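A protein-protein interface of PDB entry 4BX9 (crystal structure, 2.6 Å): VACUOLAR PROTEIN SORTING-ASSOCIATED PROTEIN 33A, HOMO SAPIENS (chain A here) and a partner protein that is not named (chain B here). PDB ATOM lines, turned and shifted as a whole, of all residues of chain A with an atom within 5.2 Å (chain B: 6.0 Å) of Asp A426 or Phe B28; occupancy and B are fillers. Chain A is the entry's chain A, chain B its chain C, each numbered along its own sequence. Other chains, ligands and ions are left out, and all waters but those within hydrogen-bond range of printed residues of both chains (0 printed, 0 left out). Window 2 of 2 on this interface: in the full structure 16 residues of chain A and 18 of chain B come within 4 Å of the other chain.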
ATOM      1  N   LYS A 421       4.511 -15.137  17.379  1.00  0.00           N
ATOM      2  CA  LYS A 421       5.900 -15.405  17.696  1.00  0.00           C
ATOM      3  C   LYS A 421       6.749 -15.048  16.483  1.00  0.00           C
ATOM      4  O   LYS A 421       6.279 -15.220  15.358  1.00  0.00           O
ATOM      5  CB  LYS A 421       6.078 -16.865  18.137  1.00  0.00           C
ATOM      6  CG  LYS A 421       5.823 -17.033  19.633  1.00  0.00           C
ATOM      7  CD  LYS A 421       5.136 -18.327  20.058  1.00  0.00           C
ATOM      8  CE  LYS A 421       3.885 -18.000  20.883  1.00  0.00           C
ATOM      9  NZ  LYS A 421       2.935 -19.140  21.022  1.00  0.00           N
ATOM     10  N   GLN A 422       7.977 -14.552  16.734  1.00  0.00           N
ATOM     11  CA  GLN A 422       8.919 -14.221  15.686  1.00  0.00           C
ATOM     12  C   GLN A 422       8.941 -15.198  14.523  1.00  0.00           C
ATOM     13  O   GLN A 422       8.874 -14.793  13.369  1.00  0.00           O
ATOM     14  CB  GLN A 422      10.353 -14.086  16.219  1.00  0.00           C
ATOM     15  CG  GLN A 422      10.742 -12.672  16.687  1.00  0.00           C
ATOM     16  CD  GLN A 422      10.529 -11.574  15.637  1.00  0.00           C
ATOM     17  OE1 GLN A 422      10.145 -10.457  15.968  1.00  0.00           O
ATOM     18  NE2 GLN A 422      10.776 -11.893  14.370  1.00  0.00           N
ATOM     19  N   LYS A 423       9.043 -16.477  14.808  1.00  0.00           N
ATOM     20  CA  LYS A 423       9.233 -17.480  13.747  1.00  0.00           C
ATOM     21  C   LYS A 423       8.048 -17.539  12.817  1.00  0.00           C
ATOM     22  O   LYS A 423       8.199 -17.661  11.623  1.00  0.00           O
ATOM     23  CB  LYS A 423       9.479 -18.874  14.347  1.00  0.00           C
ATOM     24  CG  LYS A 423      10.651 -18.874  15.303  1.00  0.00           C
ATOM     25  CD  LYS A 423      11.247 -20.265  15.503  1.00  0.00           C
ATOM     26  CE  LYS A 423      12.712 -20.160  15.937  1.00  0.00           C
ATOM     27  NZ  LYS A 423      13.137 -21.419  16.604  1.00  0.00           N
ATOM     28  N   VAL A 424       6.863 -17.473  13.394  1.00  0.00           N
ATOM     29  CA  VAL A 424       5.640 -17.508  12.639  1.00  0.00           C
ATOM     30  C   VAL A 424       5.526 -16.246  11.825  1.00  0.00           C
ATOM     31  O   VAL A 424       5.216 -16.273  10.657  1.00  0.00           O
ATOM     32  CB  VAL A 424       4.413 -17.697  13.595  1.00  0.00           C
ATOM     33  CG1 VAL A 424       3.097 -17.508  12.881  1.00  0.00           C
ATOM     34  CG2 VAL A 424       4.444 -19.086  14.238  1.00  0.00           C
ATOM     35  N   LEU A 425       5.733 -15.120  12.447  1.00  0.00           N
ATOM     36  CA  LEU A 425       5.556 -13.810  11.745  1.00  0.00           C
ATOM     37  C   LEU A 425       6.486 -13.704  10.546  1.00  0.00           C
ATOM     38  O   LEU A 425       6.050 -13.397   9.445  1.00  0.00           O
ATOM     39  CB  LEU A 425       5.787 -12.661  12.722  1.00  0.00           C
ATOM     40  CG  LEU A 425       5.988 -11.278  12.100  1.00  0.00           C
ATOM     41  CD1 LEU A 425       4.708 -10.895  11.391  1.00  0.00           C
ATOM     42  CD2 LEU A 425       6.401 -10.247  13.139  1.00  0.00           C
ATOM     43  N   ASP A 426       7.748 -14.036  10.787  1.00  0.00           N
ATOM     44  CA  ASP A 426       8.794 -14.077   9.770  1.00  0.00           C
ATOM     45  C   ASP A 426       8.518 -15.090   8.644  1.00  0.00           C
ATOM     46  O   ASP A 426       8.878 -14.873   7.507  1.00  0.00           O
ATOM     47  CB  ASP A 426      10.163 -14.390  10.417  1.00  0.00           C
ATOM     48  CG  ASP A 426      10.799 -13.168  11.173  1.00  0.00           C
ATOM     49  OD1 ASP A 426      10.237 -12.035  11.262  1.00  0.00           O
ATOM     50  OD2 ASP A 426      11.907 -13.355  11.696  1.00  0.00           O
ATOM     51  N   TYR A 427       7.869 -16.194   8.954  1.00  0.00           N
ATOM     52  CA  TYR A 427       7.571 -17.203   7.943  1.00  0.00           C
ATOM     53  C   TYR A 427       6.490 -16.663   6.999  1.00  0.00           C
ATOM     54  O   TYR A 427       6.636 -16.615   5.788  1.00  0.00           O
ATOM     55  CB  TYR A 427       7.117 -18.440   8.662  1.00  0.00           C
ATOM     56  CG  TYR A 427       6.954 -19.552   7.757  1.00  0.00           C
ATOM     57  CD1 TYR A 427       5.739 -19.754   7.097  1.00  0.00           C
ATOM     58  CD2 TYR A 427       7.994 -20.464   7.578  1.00  0.00           C
ATOM     59  CE1 TYR A 427       5.605 -20.784   6.232  1.00  0.00           C
ATOM     60  CE2 TYR A 427       7.856 -21.529   6.725  1.00  0.00           C
ATOM     61  CZ  TYR A 427       6.660 -21.659   6.051  1.00  0.00           C
ATOM     62  OH  TYR A 427       6.470 -22.697   5.207  1.00  0.00           O
ATOM     63  N   TYR A 428       5.414 -16.172   7.574  1.00  0.00           N
ATOM     64  CA  TYR A 428       4.384 -15.442   6.806  1.00  0.00           C
ATOM     65  C   TYR A 428       4.984 -14.347   5.955  1.00  0.00           C
ATOM     66  O   TYR A 428       4.686 -14.273   4.778  1.00  0.00           O
ATOM     67  CB  TYR A 428       3.314 -14.860   7.726  1.00  0.00           C
ATOM     68  CG  TYR A 428       2.246 -15.846   8.240  1.00  0.00           C
ATOM     69  CD1 TYR A 428       1.744 -16.860   7.455  1.00  0.00           C
ATOM     70  CD2 TYR A 428       1.682 -15.688   9.492  1.00  0.00           C
ATOM     71  CE1 TYR A 428       0.743 -17.712   7.917  1.00  0.00           C
ATOM     72  CE2 TYR A 428       0.664 -16.527   9.963  1.00  0.00           C
ATOM     73  CZ  TYR A 428       0.191 -17.542   9.174  1.00  0.00           C
ATOM     74  OH  TYR A 428      -0.817 -18.388   9.638  1.00  0.00           O
ATOM     75  N   LYS A 429       5.885 -13.531   6.516  1.00  0.00           N
ATOM     76  CA  LYS A 429       6.417 -12.393   5.753  1.00  0.00           C
ATOM     77  C   LYS A 429       7.285 -12.792   4.569  1.00  0.00           C
ATOM     78  O   LYS A 429       7.146 -12.261   3.460  1.00  0.00           O
ATOM     79  CB  LYS A 429       7.160 -11.410   6.662  1.00  0.00           C
ATOM     80  CG  LYS A 429       6.206 -10.708   7.632  1.00  0.00           C
ATOM     81  CD  LYS A 429       6.768  -9.465   8.239  1.00  0.00           C
ATOM     82  CE  LYS A 429       7.873  -9.759   9.196  1.00  0.00           C
ATOM     83  NZ  LYS A 429       8.556  -8.492   9.448  1.00  0.00           N
ATOM     84  N   ARG A 430       8.164 -13.744   4.786  1.00  0.00           N
ATOM     85  CA  ARG A 430       9.020 -14.214   3.692  1.00  0.00           C
ATOM     86  C   ARG A 430       8.188 -14.752   2.528  1.00  0.00           C
ATOM     87  O   ARG A 430       8.445 -14.414   1.391  1.00  0.00           O
ATOM     88  CB  ARG A 430       9.981 -15.247   4.226  1.00  0.00           C
ATOM     89  CG  ARG A 430      10.961 -15.827   3.254  1.00  0.00           C
ATOM     90  CD  ARG A 430      11.795 -16.812   4.029  1.00  0.00           C
ATOM     91  NE  ARG A 430      12.545 -17.612   3.078  1.00  0.00           N
ATOM     92  CZ  ARG A 430      13.674 -17.216   2.501  1.00  0.00           C
ATOM     93  NH1 ARG A 430      14.208 -16.031   2.796  1.00  0.00           N
ATOM     94  NH2 ARG A 430      14.257 -18.006   1.606  1.00  0.00           N
ATOM     95  N   GLU A 431       7.150 -15.532   2.816  1.00  0.00           N
ATOM     96  CA  GLU A 431       6.351 -16.095   1.733  1.00  0.00           C
ATOM     97  C   GLU A 431       5.467 -15.050   1.065  1.00  0.00           C
ATOM     98  O   GLU A 431       5.287 -15.097  -0.151  1.00  0.00           O
ATOM     99  CB  GLU A 431       5.613 -17.381   2.087  1.00  0.00           C
ATOM    100  CG  GLU A 431       4.714 -17.416   3.286  1.00  0.00           C
ATOM    101  CD  GLU A 431       4.091 -18.770   3.366  1.00  0.00           C
ATOM    102  OE1 GLU A 431       4.642 -19.666   2.686  1.00  0.00           O
ATOM    103  OE2 GLU A 431       3.073 -18.949   4.073  1.00  0.00           O
ATOM    104  N   LEU A 433       6.474 -11.777   0.680  1.00  0.00           N
ATOM    105  CA  LEU A 433       7.411 -11.090  -0.225  1.00  0.00           C
ATOM    106  C   LEU A 433       7.857 -11.908  -1.440  1.00  0.00           C
ATOM    107  O   LEU A 433       8.023 -11.386  -2.536  1.00  0.00           O
ATOM    108  CB  LEU A 433       8.662 -10.566   0.509  1.00  0.00           C
ATOM    109  CG  LEU A 433       8.421  -9.628   1.701  1.00  0.00           C
ATOM    110  CD1 LEU A 433       9.737  -9.274   2.398  1.00  0.00           C
ATOM    111  CD2 LEU A 433       7.641  -8.366   1.348  1.00  0.00           C
ATOM    112  N   ILE A 441       7.271  -4.998   1.427  1.00  0.00           N
ATOM    113  CA  ILE A 441       7.822  -4.889   2.737  1.00  0.00           C
ATOM    114  C   ILE A 441       7.363  -3.575   3.399  1.00  0.00           C
ATOM    115  O   ILE A 441       7.213  -3.472   4.613  1.00  0.00           O
ATOM    116  CB  ILE A 441       9.359  -5.004   2.752  1.00  0.00           C
ATOM    117  CG1 ILE A 441       9.794  -5.254   4.195  1.00  0.00           C
ATOM    118  CG2 ILE A 441      10.049  -3.742   2.163  1.00  0.00           C
ATOM    119  CD1 ILE A 441      11.204  -5.777   4.296  1.00  0.00           C
ATOM    120  N   ASN B  26      16.629  -4.090  12.380  1.00  0.00           N
ATOM    121  CA  ASN B  26      15.501  -4.770  11.800  1.00  0.00           C
ATOM    122  C   ASN B  26      16.082  -5.872  10.896  1.00  0.00           C
ATOM    123  O   ASN B  26      16.309  -5.716   9.671  1.00  0.00           O
ATOM    124  CB  ASN B  26      14.549  -3.728  11.158  1.00  0.00           C
ATOM    125  CG  ASN B  26      13.394  -4.350  10.419  1.00  0.00           C
ATOM    126  OD1 ASN B  26      13.382  -5.536  10.237  1.00  0.00           O
ATOM    127  ND2 ASN B  26      12.494  -3.542   9.900  1.00  0.00           N
ATOM    128  N   GLU B  27      16.371  -6.997  11.535  1.00  0.00           N
ATOM    129  CA  GLU B  27      17.081  -8.042  10.864  1.00  0.00           C
ATOM    130  C   GLU B  27      16.323  -8.620   9.682  1.00  0.00           C
ATOM    131  O   GLU B  27      16.904  -8.823   8.608  1.00  0.00           O
ATOM    132  CB  GLU B  27      17.376  -9.143  11.846  1.00  0.00           C
ATOM    133  CG  GLU B  27      18.262 -10.230  11.246  1.00  0.00           C
ATOM    134  CD  GLU B  27      19.760  -9.944  11.305  1.00  0.00           C
ATOM    135  OE1 GLU B  27      20.196  -8.765  11.576  1.00  0.00           O
ATOM    136  OE2 GLU B  27      20.506 -10.950  11.120  1.00  0.00           O
ATOM    137  N   PHE B  28      15.032  -8.889   9.858  1.00  0.00           N
ATOM    138  CA  PHE B  28      14.238  -9.460   8.767  1.00  0.00           C
ATOM    139  C   PHE B  28      14.294  -8.594   7.528  1.00  0.00           C
ATOM    140  O   PHE B  28      14.542  -9.092   6.438  1.00  0.00           O
ATOM    141  CB  PHE B  28      12.790  -9.686   9.159  1.00  0.00           C
ATOM    142  CG  PHE B  28      11.995 -10.246   8.058  1.00  0.00           C
ATOM    143  CD1 PHE B  28      11.926 -11.649   7.850  1.00  0.00           C
ATOM    144  CD2 PHE B  28      11.368  -9.411   7.156  1.00  0.00           C
ATOM    145  CE1 PHE B  28      11.186 -12.175   6.785  1.00  0.00           C
ATOM    146  CE2 PHE B  28      10.646  -9.933   6.100  1.00  0.00           C
ATOM    147  CZ  PHE B  28      10.559 -11.331   5.907  1.00  0.00           C
ATOM    148  N   ALA B  29      14.108  -7.300   7.712  1.00  0.00           N
ATOM    149  CA  ALA B  29      14.150  -6.371   6.587  1.00  0.00           C
ATOM    150  C   ALA B  29      15.484  -6.368   5.824  1.00  0.00           C
ATOM    151  O   ALA B  29      15.509  -6.404   4.582  1.00  0.00           O
ATOM    152  CB  ALA B  29      13.785  -4.925   7.041  1.00  0.00           C
ATOM    153  N   ALA B  30      16.577  -6.279   6.576  1.00  0.00           N
ATOM    154  CA  ALA B  30      17.917  -6.358   5.965  1.00  0.00           C
ATOM    155  C   ALA B  30      18.070  -7.602   5.077  1.00  0.00           C
ATOM    156  O   ALA B  30      18.551  -7.487   3.911  1.00  0.00           O
ATOM    157  CB  ALA B  30      19.026  -6.361   7.029  1.00  0.00           C
ATOM    158  N   LYS B  31      17.672  -8.771   5.606  1.00  0.00           N
ATOM    159  CA  LYS B  31      17.889 -10.009   4.853  1.00  0.00           C
ATOM    160  C   LYS B  31      17.041 -10.035   3.615  1.00  0.00           C
ATOM    161  O   LYS B  31      17.514 -10.446   2.554  1.00  0.00           O
ATOM    162  CB  LYS B  31      17.575 -11.229   5.675  1.00  0.00           C
ATOM    163  CG  LYS B  31      18.482 -11.392   6.870  1.00  0.00           C
ATOM    164  CD  LYS B  31      19.838 -12.002   6.494  1.00  0.00           C
ATOM    165  CE  LYS B  31      20.899 -11.583   7.470  1.00  0.00           C
ATOM    166  NZ  LYS B  31      22.195 -11.430   6.749  1.00  0.00           N
ATOM    167  N   ALA B  32      15.785  -9.617   3.760  1.00  0.00           N
ATOM    168  CA  ALA B  32      14.887  -9.543   2.642  1.00  0.00           C
ATOM    169  C   ALA B  32      15.408  -8.628   1.548  1.00  0.00           C
ATOM    170  O   ALA B  32      15.212  -8.859   0.378  1.00  0.00           O
ATOM    171  CB  ALA B  32      13.550  -9.050   3.111  1.00  0.00           C
ATOM    172  N   THR B  33      16.030  -7.538   1.943  1.00  0.00           N
ATOM    173  CA  THR B  33      16.583  -6.584   1.001  1.00  0.00           C
ATOM    174  C   THR B  33      17.799  -7.229   0.320  1.00  0.00           C
ATOM    175  O   THR B  33      17.911  -7.180  -0.901  1.00  0.00           O
ATOM    176  CB  THR B  33      16.961  -5.319   1.752  1.00  0.00           C
ATOM    177  OG1 THR B  33      15.786  -4.704   2.274  1.00  0.00           O
ATOM    178  CG2 THR B  33      17.713  -4.348   0.839  1.00  0.00           C
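The side-chain amide oxygen (OD1) of Asn B26 lies within hydrogen-bond range of the backbone NH (N) of Ala B29, at 3.2 Å. OD1 of Asp A426 is in hydrogen-bond range of NE2 of Gln A422. The side-chain hydroxyl of Thr B33 is in hydrogen-bond range of the backbone carbonyl oxygen of Ala B29, 2.9 Å away.
Asp A426 touches Phe B28. Lys A429 touches Phe B28. N of Arg A430 touches CZ of Phe B28, at 3.6 Å. Leu A433 touches Phe B28. CB of Ala B32 touches CD1 of Leu A433, at 3.9 Å. CD1 of Ile A441 touches CA of Ala B29, 3.8 Å away.
Of chain B, only Phe B28 comes within 4 Å of Asp A426. Of the printed residues of chain A, Phe B28 touches Asp A426, Lys A429, Arg A430 and Leu A433. Printed residues of chain B within 4 Å of Ile A441: Ala B29 (3.8 Å). Of the printed residues of chain B, Arg A430 touches Phe B28 (3.6 Å). Printed residues of chain B within 4 Å of Leu A433: Phe B28 and Ala B32. Glu B27 touches none of the printed residues of chain A. Thr B33 touches none of the printed residues of chain A. The nearest printed residue of chain B that does not touch Asp A426 is Glu B27 (6.8 Å). The nearest residue of chain A that does not touch Phe B28 is Ile A441 (4.6 Å).
Of the 8 printed residues of chain B, 3 touch a printed residue of chain A. Hydrophobic or aromatic side chains of chain B within 4 Å of the printed part of chain A: Phe B28, Ala B29 and Ala B32. Hydrophobic or aromatic side chains of chain A within 4 Å of the printed part of chain B: Leu A433 and Ile A441. Among the printed residues, 6 pairs touch across the chains. Among the printed residues, no Asp or Glu carboxylate lies within 4 Å of a Lys or Arg side-chain nitrogen of the other chain.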
